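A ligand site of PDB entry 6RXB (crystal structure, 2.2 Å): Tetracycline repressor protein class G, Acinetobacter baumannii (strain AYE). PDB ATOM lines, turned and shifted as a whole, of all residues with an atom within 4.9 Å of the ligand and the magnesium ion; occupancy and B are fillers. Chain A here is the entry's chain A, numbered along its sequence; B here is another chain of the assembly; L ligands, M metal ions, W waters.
Merely in contact with the ligand: Leu 60, Phe 86, Thr 103, Pro 105, Asn 109, Ala 113, Val 131, Leu 134, Ser 138 and Phe 176 of chain B.
Hydrophobic or aromatic side chains within 4 Å of the ligand: Leu 60, His 64, Phe 86, His 100, Pro 105, Ala 113, Val 131 and Phe 176 of chain B.
Of the 23 residues printed, 15 come within 4 Å of the ligand.
Water W2 lies within hydrogen-bond range of the side-chain carboxylate (OE2) of Glu 147 of chain B (2.7 Å) and the side-chain hydroxyl (OG) of Ser 138 (3.1 Å).
Water W4 bridges OE1 of Glu 147 of chain B (2.5 Å) and O of Thr 103 (2.6 Å).
Water W3 lies within hydrogen-bond range of the backbone carbonyl oxygen of Ser 67, an oxygen (O1) of the ligand and the side-chain amide nitrogen of Asn 82.
The backbone carbonyl oxygen of Asn 109 is in hydrogen-bond range of the side-chain hydroxyl of Thr 112.
The backbone carbonyl oxygen (O) of His 100 is in hydrogen-bond range of the side-chain hydroxyl (OG1) of Thr 103 (2.5 Å).
The backbone NH of Phe 86 lies within hydrogen-bond range of a ring nitrogen (ND1) of His 64, at 3.3 Å.
O of Arg 135 sits at hydrogen-bond distance from OG of Ser 138, 2.6 Å away.
The side-chain amide nitrogen (ND2) of Asn 82 is in hydrogen-bond range of the backbone carbonyl oxygen (O) of Arg 66 (2.7 Å).
Residues that only touch the magnesium ion: Thr 103 (3.9 Å) and Glu 147 of chain B (3.9 Å).
Within 4 Å of the magnesium ion: His 100, Thr 103 and Glu 147 of chain B.
The nearest printed residue that does not touch the magnesium ion is Ser 138 (4.8 Å).
The magnesium ion is bound by water W4 (1.9 Å), water W2 (1.9 Å), an oxygen (O6) of the ligand (2.0 Å), water W1 (2.2 Å), an oxygen (O5) of the ligand (2.3 Å) and a ring nitrogen (NE2) of His 100 (2.4 Å).
The magnesium ion has six donor atoms within binding distance.
OG of Ser 67 sits at hydrogen-bond distance from O1 of the ligand, 3.2 Å away.
An oxygen (O3) of the ligand sits at hydrogen-bond distance from a ring nitrogen (NE2) of His 64 (2.7 Å).
O3 of the ligand lies within hydrogen-bond range of ND2 of Asn 82 (2.8 Å).
NE of Arg 104 lies within hydrogen-bond range of O7 of the ligand (2.9 Å).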
ATOM      1  N   LEU A  60       4.973  -5.468  28.794  1.00  0.00           N
ATOM      2  CA  LEU A  60       5.175  -6.171  27.493  1.00  0.00           C
ATOM      3  C   LEU A  60       5.727  -5.192  26.457  1.00  0.00           C
ATOM      4  O   LEU A  60       6.689  -5.566  25.748  1.00  0.00           O
ATOM      5  CB  LEU A  60       3.843  -6.774  27.035  1.00  0.00           C
ATOM      6  CG  LEU A  60       3.211  -7.796  27.994  1.00  0.00           C
ATOM      7  CD1 LEU A  60       1.917  -8.349  27.419  1.00  0.00           C
ATOM      8  CD2 LEU A  60       4.176  -8.922  28.307  1.00  0.00           C
ATOM      9  N   HIS A  64       8.892  -7.235  26.349  1.00  0.00           N
ATOM     10  CA  HIS A  64       8.465  -8.318  25.417  1.00  0.00           C
ATOM     11  C   HIS A  64       8.876  -7.949  23.978  1.00  0.00           C
ATOM     12  O   HIS A  64       8.071  -7.298  23.282  1.00  0.00           O
ATOM     13  CB  HIS A  64       6.970  -8.611  25.568  1.00  0.00           C
ATOM     14  CG  HIS A  64       6.506  -9.832  24.849  1.00  0.00           C
ATOM     15  ND1 HIS A  64       7.346 -10.906  24.611  1.00  0.00           N
ATOM     16  CD2 HIS A  64       5.300 -10.167  24.336  1.00  0.00           C
ATOM     17  CE1 HIS A  64       6.677 -11.843  23.965  1.00  0.00           C
ATOM     18  NE2 HIS A  64       5.424 -11.413  23.792  1.00  0.00           N
ATOM     19  N   ARG A  66      10.004 -10.214  21.438  1.00  0.00           N
ATOM     20  CA  ARG A  66       9.618 -11.245  20.433  1.00  0.00           C
ATOM     21  C   ARG A  66       8.094 -11.472  20.480  1.00  0.00           C
ATOM     22  O   ARG A  66       7.683 -12.598  20.811  1.00  0.00           O
ATOM     23  CB  ARG A  66      10.394 -12.541  20.675  1.00  0.00           C
ATOM     24  CG  ARG A  66      11.904 -12.411  20.522  1.00  0.00           C
ATOM     25  CD  ARG A  66      12.353 -11.829  19.195  1.00  0.00           C
ATOM     26  NE  ARG A  66      11.489 -12.181  18.077  1.00  0.00           N
ATOM     27  CZ  ARG A  66      11.448 -13.374  17.480  1.00  0.00           C
ATOM     28  NH1 ARG A  66      10.604 -13.578  16.479  1.00  0.00           N
ATOM     29  NH2 ARG A  66      12.228 -14.365  17.881  1.00  0.00           N
ATOM     30  N   SER A  67       7.316 -10.448  20.135  1.00  0.00           N
ATOM     31  CA  SER A  67       5.832 -10.503  20.017  1.00  0.00           C
ATOM     32  C   SER A  67       5.443 -11.106  18.659  1.00  0.00           C
ATOM     33  O   SER A  67       4.464 -11.878  18.617  1.00  0.00           O
ATOM     34  CB  SER A  67       5.209  -9.132  20.195  1.00  0.00           C
ATOM     35  OG  SER A  67       5.303  -8.715  21.546  1.00  0.00           O
ATOM     36  N   ASN A  82       9.268 -16.468  21.751  1.00  0.00           N
ATOM     37  CA  ASN A  82       8.059 -15.691  22.158  1.00  0.00           C
ATOM     38  C   ASN A  82       7.749 -15.971  23.629  1.00  0.00           C
ATOM     39  O   ASN A  82       7.505 -15.002  24.377  1.00  0.00           O
ATOM     40  CB  ASN A  82       6.856 -16.004  21.253  1.00  0.00           C
ATOM     41  CG  ASN A  82       5.599 -15.291  21.685  1.00  0.00           C
ATOM     42  OD1 ASN A  82       4.751 -15.880  22.357  1.00  0.00           O
ATOM     43  ND2 ASN A  82       5.462 -14.029  21.314  1.00  0.00           N
ATOM     44  N   PHE A  86       8.223 -13.334  26.676  1.00  0.00           N
ATOM     45  CA  PHE A  86       7.010 -13.098  27.519  1.00  0.00           C
ATOM     46  C   PHE A  86       7.356 -13.351  28.995  1.00  0.00           C
ATOM     47  O   PHE A  86       6.974 -12.518  29.842  1.00  0.00           O
ATOM     48  CB  PHE A  86       5.848 -13.975  27.044  1.00  0.00           C
ATOM     49  CG  PHE A  86       4.586 -13.826  27.837  1.00  0.00           C
ATOM     50  CD1 PHE A  86       3.999 -12.589  28.037  1.00  0.00           C
ATOM     51  CD2 PHE A  86       3.952 -14.939  28.378  1.00  0.00           C
ATOM     52  CE1 PHE A  86       2.823 -12.455  28.775  1.00  0.00           C
ATOM     53  CE2 PHE A  86       2.783 -14.816  29.112  1.00  0.00           C
ATOM     54  CZ  PHE A  86       2.219 -13.572  29.305  1.00  0.00           C
ATOM     55  N   HIS A 100      -0.727  -9.731  35.383  1.00  0.00           N
ATOM     56  CA  HIS A 100      -1.130 -10.168  34.017  1.00  0.00           C
ATOM     57  C   HIS A 100      -2.377 -11.060  34.084  1.00  0.00           C
ATOM     58  O   HIS A 100      -3.193 -10.969  33.142  1.00  0.00           O
ATOM     59  CB  HIS A 100       0.033 -10.892  33.314  1.00  0.00           C
ATOM     60  CG  HIS A 100      -0.282 -11.268  31.903  1.00  0.00           C
ATOM     61  ND1 HIS A 100       0.007 -10.435  30.846  1.00  0.00           N
ATOM     62  CD2 HIS A 100      -0.866 -12.370  31.389  1.00  0.00           C
ATOM     63  CE1 HIS A 100      -0.381 -11.016  29.724  1.00  0.00           C
ATOM     64  NE2 HIS A 100      -0.923 -12.195  30.037  1.00  0.00           N
ATOM     65  N   THR A 103      -6.232 -10.590  32.542  1.00  0.00           N
ATOM     66  CA  THR A 103      -6.221  -9.532  31.486  1.00  0.00           C
ATOM     67  C   THR A 103      -6.533 -10.161  30.132  1.00  0.00           C
ATOM     68  O   THR A 103      -6.079 -11.306  29.897  1.00  0.00           O
ATOM     69  CB  THR A 103      -4.871  -8.789  31.428  1.00  0.00           C
ATOM     70  OG1 THR A 103      -3.853  -9.738  31.112  1.00  0.00           O
ATOM     71  CG2 THR A 103      -4.527  -8.072  32.712  1.00  0.00           C
ATOM     72  N   ARG A 104      -7.292  -9.460  29.286  1.00  0.00           N
ATOM     73  CA  ARG A 104      -7.569  -9.851  27.881  1.00  0.00           C
ATOM     74  C   ARG A 104      -6.732  -8.959  26.966  1.00  0.00           C
ATOM     75  O   ARG A 104      -6.439  -7.814  27.308  1.00  0.00           O
ATOM     76  CB  ARG A 104      -9.069  -9.737  27.571  1.00  0.00           C
ATOM     77  CG  ARG A 104      -9.909 -10.856  28.175  1.00  0.00           C
ATOM     78  CD  ARG A 104      -9.574 -12.237  27.629  1.00  0.00           C
ATOM     79  NE  ARG A 104      -8.626 -12.965  28.475  1.00  0.00           N
ATOM     80  CZ  ARG A 104      -8.932 -13.588  29.608  1.00  0.00           C
ATOM     81  NH1 ARG A 104     -10.175 -13.585  30.070  1.00  0.00           N
ATOM     82  NH2 ARG A 104      -7.987 -14.219  30.288  1.00  0.00           N
ATOM     83  N   PRO A 105      -6.318  -9.458  25.772  1.00  0.00           N
ATOM     84  CA  PRO A 105      -5.491  -8.675  24.855  1.00  0.00           C
ATOM     85  C   PRO A 105      -6.096  -7.305  24.502  1.00  0.00           C
ATOM     86  O   PRO A 105      -7.306  -7.224  24.315  1.00  0.00           O
ATOM     87  CB  PRO A 105      -5.432  -9.553  23.591  1.00  0.00           C
ATOM     88  CG  PRO A 105      -5.642 -10.961  24.110  1.00  0.00           C
ATOM     89  CD  PRO A 105      -6.616 -10.795  25.252  1.00  0.00           C
ATOM     90  N   ASN A 109      -2.596  -6.026  20.743  1.00  0.00           N
ATOM     91  CA  ASN A 109      -2.301  -7.429  21.140  1.00  0.00           C
ATOM     92  C   ASN A 109      -3.147  -8.395  20.298  1.00  0.00           C
ATOM     93  O   ASN A 109      -2.627  -9.473  19.965  1.00  0.00           O
ATOM     94  CB  ASN A 109      -2.521  -7.658  22.638  1.00  0.00           C
ATOM     95  CG  ASN A 109      -1.505  -6.944  23.514  1.00  0.00           C
ATOM     96  OD1 ASN A 109      -0.528  -6.382  23.022  1.00  0.00           O
ATOM     97  ND2 ASN A 109      -1.741  -6.968  24.814  1.00  0.00           N
ATOM     98  N   PHE A 110      -4.393  -8.015  19.974  1.00  0.00           N
ATOM     99  CA  PHE A 110      -5.297  -8.768  19.077  1.00  0.00           C
ATOM    100  C   PHE A 110      -4.679  -8.842  17.671  1.00  0.00           C
ATOM    101  O   PHE A 110      -4.779  -9.905  17.026  1.00  0.00           O
ATOM    102  CB  PHE A 110      -6.693  -8.139  19.021  1.00  0.00           C
ATOM    103  CG  PHE A 110      -7.659  -8.610  20.082  1.00  0.00           C
ATOM    104  CD1 PHE A 110      -8.001  -9.947  20.167  1.00  0.00           C
ATOM    105  CD2 PHE A 110      -8.231  -7.724  20.972  1.00  0.00           C
ATOM    106  CE1 PHE A 110      -8.892 -10.391  21.136  1.00  0.00           C
ATOM    107  CE2 PHE A 110      -9.131  -8.162  21.932  1.00  0.00           C
ATOM    108  CZ  PHE A 110      -9.451  -9.495  22.020  1.00  0.00           C
ATOM    109  N   THR A 112      -1.337  -8.599  16.931  1.00  0.00           N
ATOM    110  CA  THR A 112      -0.139  -9.463  17.073  1.00  0.00           C
ATOM    111  C   THR A 112      -0.573 -10.924  17.275  1.00  0.00           C
ATOM    112  O   THR A 112       0.127 -11.810  16.761  1.00  0.00           O
ATOM    113  CB  THR A 112       0.761  -8.993  18.232  1.00  0.00           C
ATOM    114  OG1 THR A 112       0.021  -9.080  19.444  1.00  0.00           O
ATOM    115  CG2 THR A 112       1.286  -7.577  18.038  1.00  0.00           C
ATOM    116  N   ALA A 113      -1.685 -11.141  17.989  1.00  0.00           N
ATOM    117  CA  ALA A 113      -2.295 -12.464  18.238  1.00  0.00           C
ATOM    118  C   ALA A 113      -2.767 -13.077  16.914  1.00  0.00           C
ATOM    119  O   ALA A 113      -2.506 -14.279  16.688  1.00  0.00           O
ATOM    120  CB  ALA A 113      -3.420 -12.354  19.229  1.00  0.00           C
ATOM    121  N   ILE A 117      -1.591 -16.447  15.098  1.00  0.00           N
ATOM    122  CA  ILE A 117      -2.619 -17.461  14.736  1.00  0.00           C
ATOM    123  C   ILE A 117      -2.464 -17.819  13.251  1.00  0.00           C
ATOM    124  O   ILE A 117      -2.410 -19.032  12.943  1.00  0.00           O
ATOM    125  CB  ILE A 117      -4.040 -16.966  15.058  1.00  0.00           C
ATOM    126  CG1 ILE A 117      -4.282 -16.912  16.574  1.00  0.00           C
ATOM    127  CG2 ILE A 117      -5.094 -17.815  14.361  1.00  0.00           C
ATOM    128  CD1 ILE A 117      -5.419 -16.001  16.987  1.00  0.00           C
ATOM    129  N   VAL A 131      -5.108 -21.055  18.423  1.00  0.00           N
ATOM    130  CA  VAL A 131      -5.570 -20.206  19.554  1.00  0.00           C
ATOM    131  C   VAL A 131      -5.231 -20.912  20.874  1.00  0.00           C
ATOM    132  O   VAL A 131      -4.659 -20.255  21.766  1.00  0.00           O
ATOM    133  CB  VAL A 131      -7.070 -19.887  19.450  1.00  0.00           C
ATOM    134  CG1 VAL A 131      -7.637 -19.327  20.747  1.00  0.00           C
ATOM    135  CG2 VAL A 131      -7.375 -18.956  18.291  1.00  0.00           C
ATOM    136  N   LEU A 134      -1.386 -21.003  21.684  1.00  0.00           N
ATOM    137  CA  LEU A 134      -0.893 -19.657  22.121  1.00  0.00           C
ATOM    138  C   LEU A 134      -1.386 -19.371  23.547  1.00  0.00           C
ATOM    139  O   LEU A 134      -0.584 -18.834  24.337  1.00  0.00           O
ATOM    140  CB  LEU A 134      -1.388 -18.594  21.137  1.00  0.00           C
ATOM    141  CG  LEU A 134      -0.752 -18.644  19.741  1.00  0.00           C
ATOM    142  CD1 LEU A 134      -1.495 -17.756  18.768  1.00  0.00           C
ATOM    143  CD2 LEU A 134       0.719 -18.264  19.799  1.00  0.00           C
ATOM    144  N   ARG A 135      -2.640 -19.697  23.860  1.00  0.00           N
ATOM    145  CA  ARG A 135      -3.249 -19.542  25.203  1.00  0.00           C
ATOM    146  C   ARG A 135      -2.523 -20.460  26.207  1.00  0.00           C
ATOM    147  O   ARG A 135      -2.206 -19.976  27.316  1.00  0.00           O
ATOM    148  CB  ARG A 135      -4.749 -19.854  25.194  1.00  0.00           C
ATOM    149  CG  ARG A 135      -5.634 -18.709  24.753  1.00  0.00           C
ATOM    150  CD  ARG A 135      -7.085 -18.941  25.149  1.00  0.00           C
ATOM    151  NE  ARG A 135      -7.306 -18.765  26.577  1.00  0.00           N
ATOM    152  CZ  ARG A 135      -8.366 -19.219  27.249  1.00  0.00           C
ATOM    153  NH1 ARG A 135      -9.323 -19.898  26.640  1.00  0.00           N
ATOM    154  NH2 ARG A 135      -8.466 -18.993  28.553  1.00  0.00           N
ATOM    155  N   VAL A 137       0.527 -21.719  26.105  1.00  0.00           N
ATOM    156  CA  VAL A 137       1.917 -21.221  26.316  1.00  0.00           C
ATOM    157  C   VAL A 137       1.870 -20.066  27.326  1.00  0.00           C
ATOM    158  O   VAL A 137       2.675 -20.092  28.284  1.00  0.00           O
ATOM    159  CB  VAL A 137       2.583 -20.790  24.993  1.00  0.00           C
ATOM    160  CG1 VAL A 137       3.873 -20.032  25.230  1.00  0.00           C
ATOM    161  CG2 VAL A 137       2.834 -21.986  24.085  1.00  0.00           C
ATOM    162  N   SER A 138       0.973 -19.087  27.119  1.00  0.00           N
ATOM    163  CA  SER A 138       0.804 -17.885  27.980  1.00  0.00           C
ATOM    164  C   SER A 138       0.467 -18.323  29.416  1.00  0.00           C
ATOM    165  O   SER A 138       1.073 -17.776  30.352  1.00  0.00           O
ATOM    166  CB  SER A 138      -0.235 -16.961  27.427  1.00  0.00           C
ATOM    167  OG  SER A 138      -1.540 -17.495  27.575  1.00  0.00           O
ATOM    168  N   GLU B 147      -5.546 -17.493  35.995  1.00  0.00           N
ATOM    169  CA  GLU B 147      -6.073 -16.568  34.962  1.00  0.00           C
ATOM    170  C   GLU B 147      -7.608 -16.665  34.899  1.00  0.00           C
ATOM    171  O   GLU B 147      -8.250 -15.607  34.740  1.00  0.00           O
ATOM    172  CB  GLU B 147      -5.457 -16.872  33.590  1.00  0.00           C
ATOM    173  CG  GLU B 147      -3.974 -16.529  33.514  1.00  0.00           C
ATOM    174  CD  GLU B 147      -3.595 -15.616  32.364  1.00  0.00           C
ATOM    175  OE1 GLU B 147      -4.261 -14.570  32.199  1.00  0.00           O
ATOM    176  OE2 GLU B 147      -2.630 -15.940  31.644  1.00  0.00           O
ATOM    177  N   VAL B 163     -14.789 -12.052  24.578  1.00  0.00           N
ATOM    178  CA  VAL B 163     -13.529 -11.954  23.768  1.00  0.00           C
ATOM    179  C   VAL B 163     -13.910 -11.822  22.282  1.00  0.00           C
ATOM    180  O   VAL B 163     -13.216 -11.074  21.570  1.00  0.00           O
ATOM    181  CB  VAL B 163     -12.602 -13.158  24.002  1.00  0.00           C
ATOM    182  CG1 VAL B 163     -11.268 -13.002  23.264  1.00  0.00           C
ATOM    183  CG2 VAL B 163     -12.352 -13.416  25.482  1.00  0.00           C
ATOM    184  N   PHE B 176     -13.707 -16.938  17.622  1.00  0.00           N
ATOM    185  CA  PHE B 176     -14.030 -16.899  19.074  1.00  0.00           C
ATOM    186  C   PHE B 176     -15.493 -17.279  19.298  1.00  0.00           C
ATOM    187  O   PHE B 176     -15.799 -17.851  20.366  1.00  0.00           O
ATOM    188  CB  PHE B 176     -13.725 -15.520  19.677  1.00  0.00           C
ATOM    189  CG  PHE B 176     -12.286 -15.079  19.617  1.00  0.00           C
ATOM    190  CD1 PHE B 176     -11.249 -15.996  19.608  1.00  0.00           C
ATOM    191  CD2 PHE B 176     -11.967 -13.726  19.592  1.00  0.00           C
ATOM    192  CE1 PHE B 176      -9.930 -15.576  19.555  1.00  0.00           C
ATOM    193  CE2 PHE B 176     -10.648 -13.310  19.548  1.00  0.00           C
ATOM    194  CZ  PHE B 176      -9.626 -14.239  19.522  1.00  0.00           C
HETATM  195  O1  LIG L   1       2.864 -10.676  22.358  1.00  0.00           O
HETATM  196  C1  LIG L   1       2.069 -10.708  23.276  1.00  0.00           C
HETATM  197  N1  LIG L   1       1.579  -9.431  23.835  1.00  0.00           N
HETATM  198  C2  LIG L   1       1.585 -12.019  23.798  1.00  0.00           C
HETATM  199  C3  LIG L   1       0.457 -12.108  24.673  1.00  0.00           C
HETATM  200  O2  LIG L   1      -0.240 -11.127  24.966  1.00  0.00           O
HETATM  201  C4  LIG L   1       2.243 -13.197  23.463  1.00  0.00           C
HETATM  202  O3  LIG L   1       3.512 -13.238  23.095  1.00  0.00           O
HETATM  203  C5  LIG L   1       1.548 -14.532  23.410  1.00  0.00           C
HETATM  204  N2  LIG L   1       2.470 -15.638  23.760  1.00  0.00           N
HETATM  205  C6  LIG L   1       2.024 -16.975  23.373  1.00  0.00           C
HETATM  206  C7  LIG L   1       3.045 -15.648  25.112  1.00  0.00           C
HETATM  207  C8  LIG L   1       0.237 -14.592  24.222  1.00  0.00           C
HETATM  208  C9  LIG L   1       0.084 -13.487  25.270  1.00  0.00           C
HETATM  209  O4  LIG L   1       0.993 -13.754  26.339  1.00  0.00           O
HETATM  210  C10 LIG L   1      -1.301 -13.467  25.873  1.00  0.00           C
HETATM  211  O5  LIG L   1      -1.385 -12.790  27.018  1.00  0.00           O
HETATM  212  C11 LIG L   1      -2.389 -14.072  25.320  1.00  0.00           C
HETATM  213  C12 LIG L   1      -2.294 -14.819  24.015  1.00  0.00           C
HETATM  214  C13 LIG L   1      -0.972 -14.593  23.284  1.00  0.00           C
HETATM  215  C14 LIG L   1      -3.668 -14.025  25.993  1.00  0.00           C
HETATM  216  O6  LIG L   1      -3.752 -13.766  27.236  1.00  0.00           O
HETATM  217  C15 LIG L   1      -4.871 -14.292  25.217  1.00  0.00           C
HETATM  218  C16 LIG L   1      -4.794 -14.471  23.823  1.00  0.00           C
HETATM  219  C17 LIG L   1      -3.477 -14.418  23.128  1.00  0.00           C
HETATM  220  C18 LIG L   1      -6.132 -14.356  25.845  1.00  0.00           C
HETATM  221  O7  LIG L   1      -6.278 -14.184  27.178  1.00  0.00           O
HETATM  222  C19 LIG L   1      -7.276 -14.605  25.090  1.00  0.00           C
HETATM  223  C20 LIG L   1      -7.188 -14.790  23.727  1.00  0.00           C
HETATM  224  C21 LIG L   1      -5.970 -14.729  23.084  1.00  0.00           C
HETATM  225  N3  LIG L   1      -5.884 -14.915  21.699  1.00  0.00           N
HETATM  226  C22 LIG L   1      -6.386 -13.894  20.794  1.00  0.00           C
HETATM  227  C23 LIG L   1      -5.647 -16.235  21.140  1.00  0.00           C
HETATM  228 MG    MG M   1      -2.790 -13.079  28.868  1.00  0.00          MG
HETATM  229  O   HOH W   1      -3.462 -11.078  28.340  1.00  0.00           O
HETATM  230  O   HOH W   2      -2.317 -14.934  29.206  1.00  0.00           O
HETATM  231  O   HOH W   3       2.560 -12.497  20.367  1.00  0.00           O
HETATM  232  O   HOH W   4      -4.234 -13.086  30.128  1.00  0.00           O
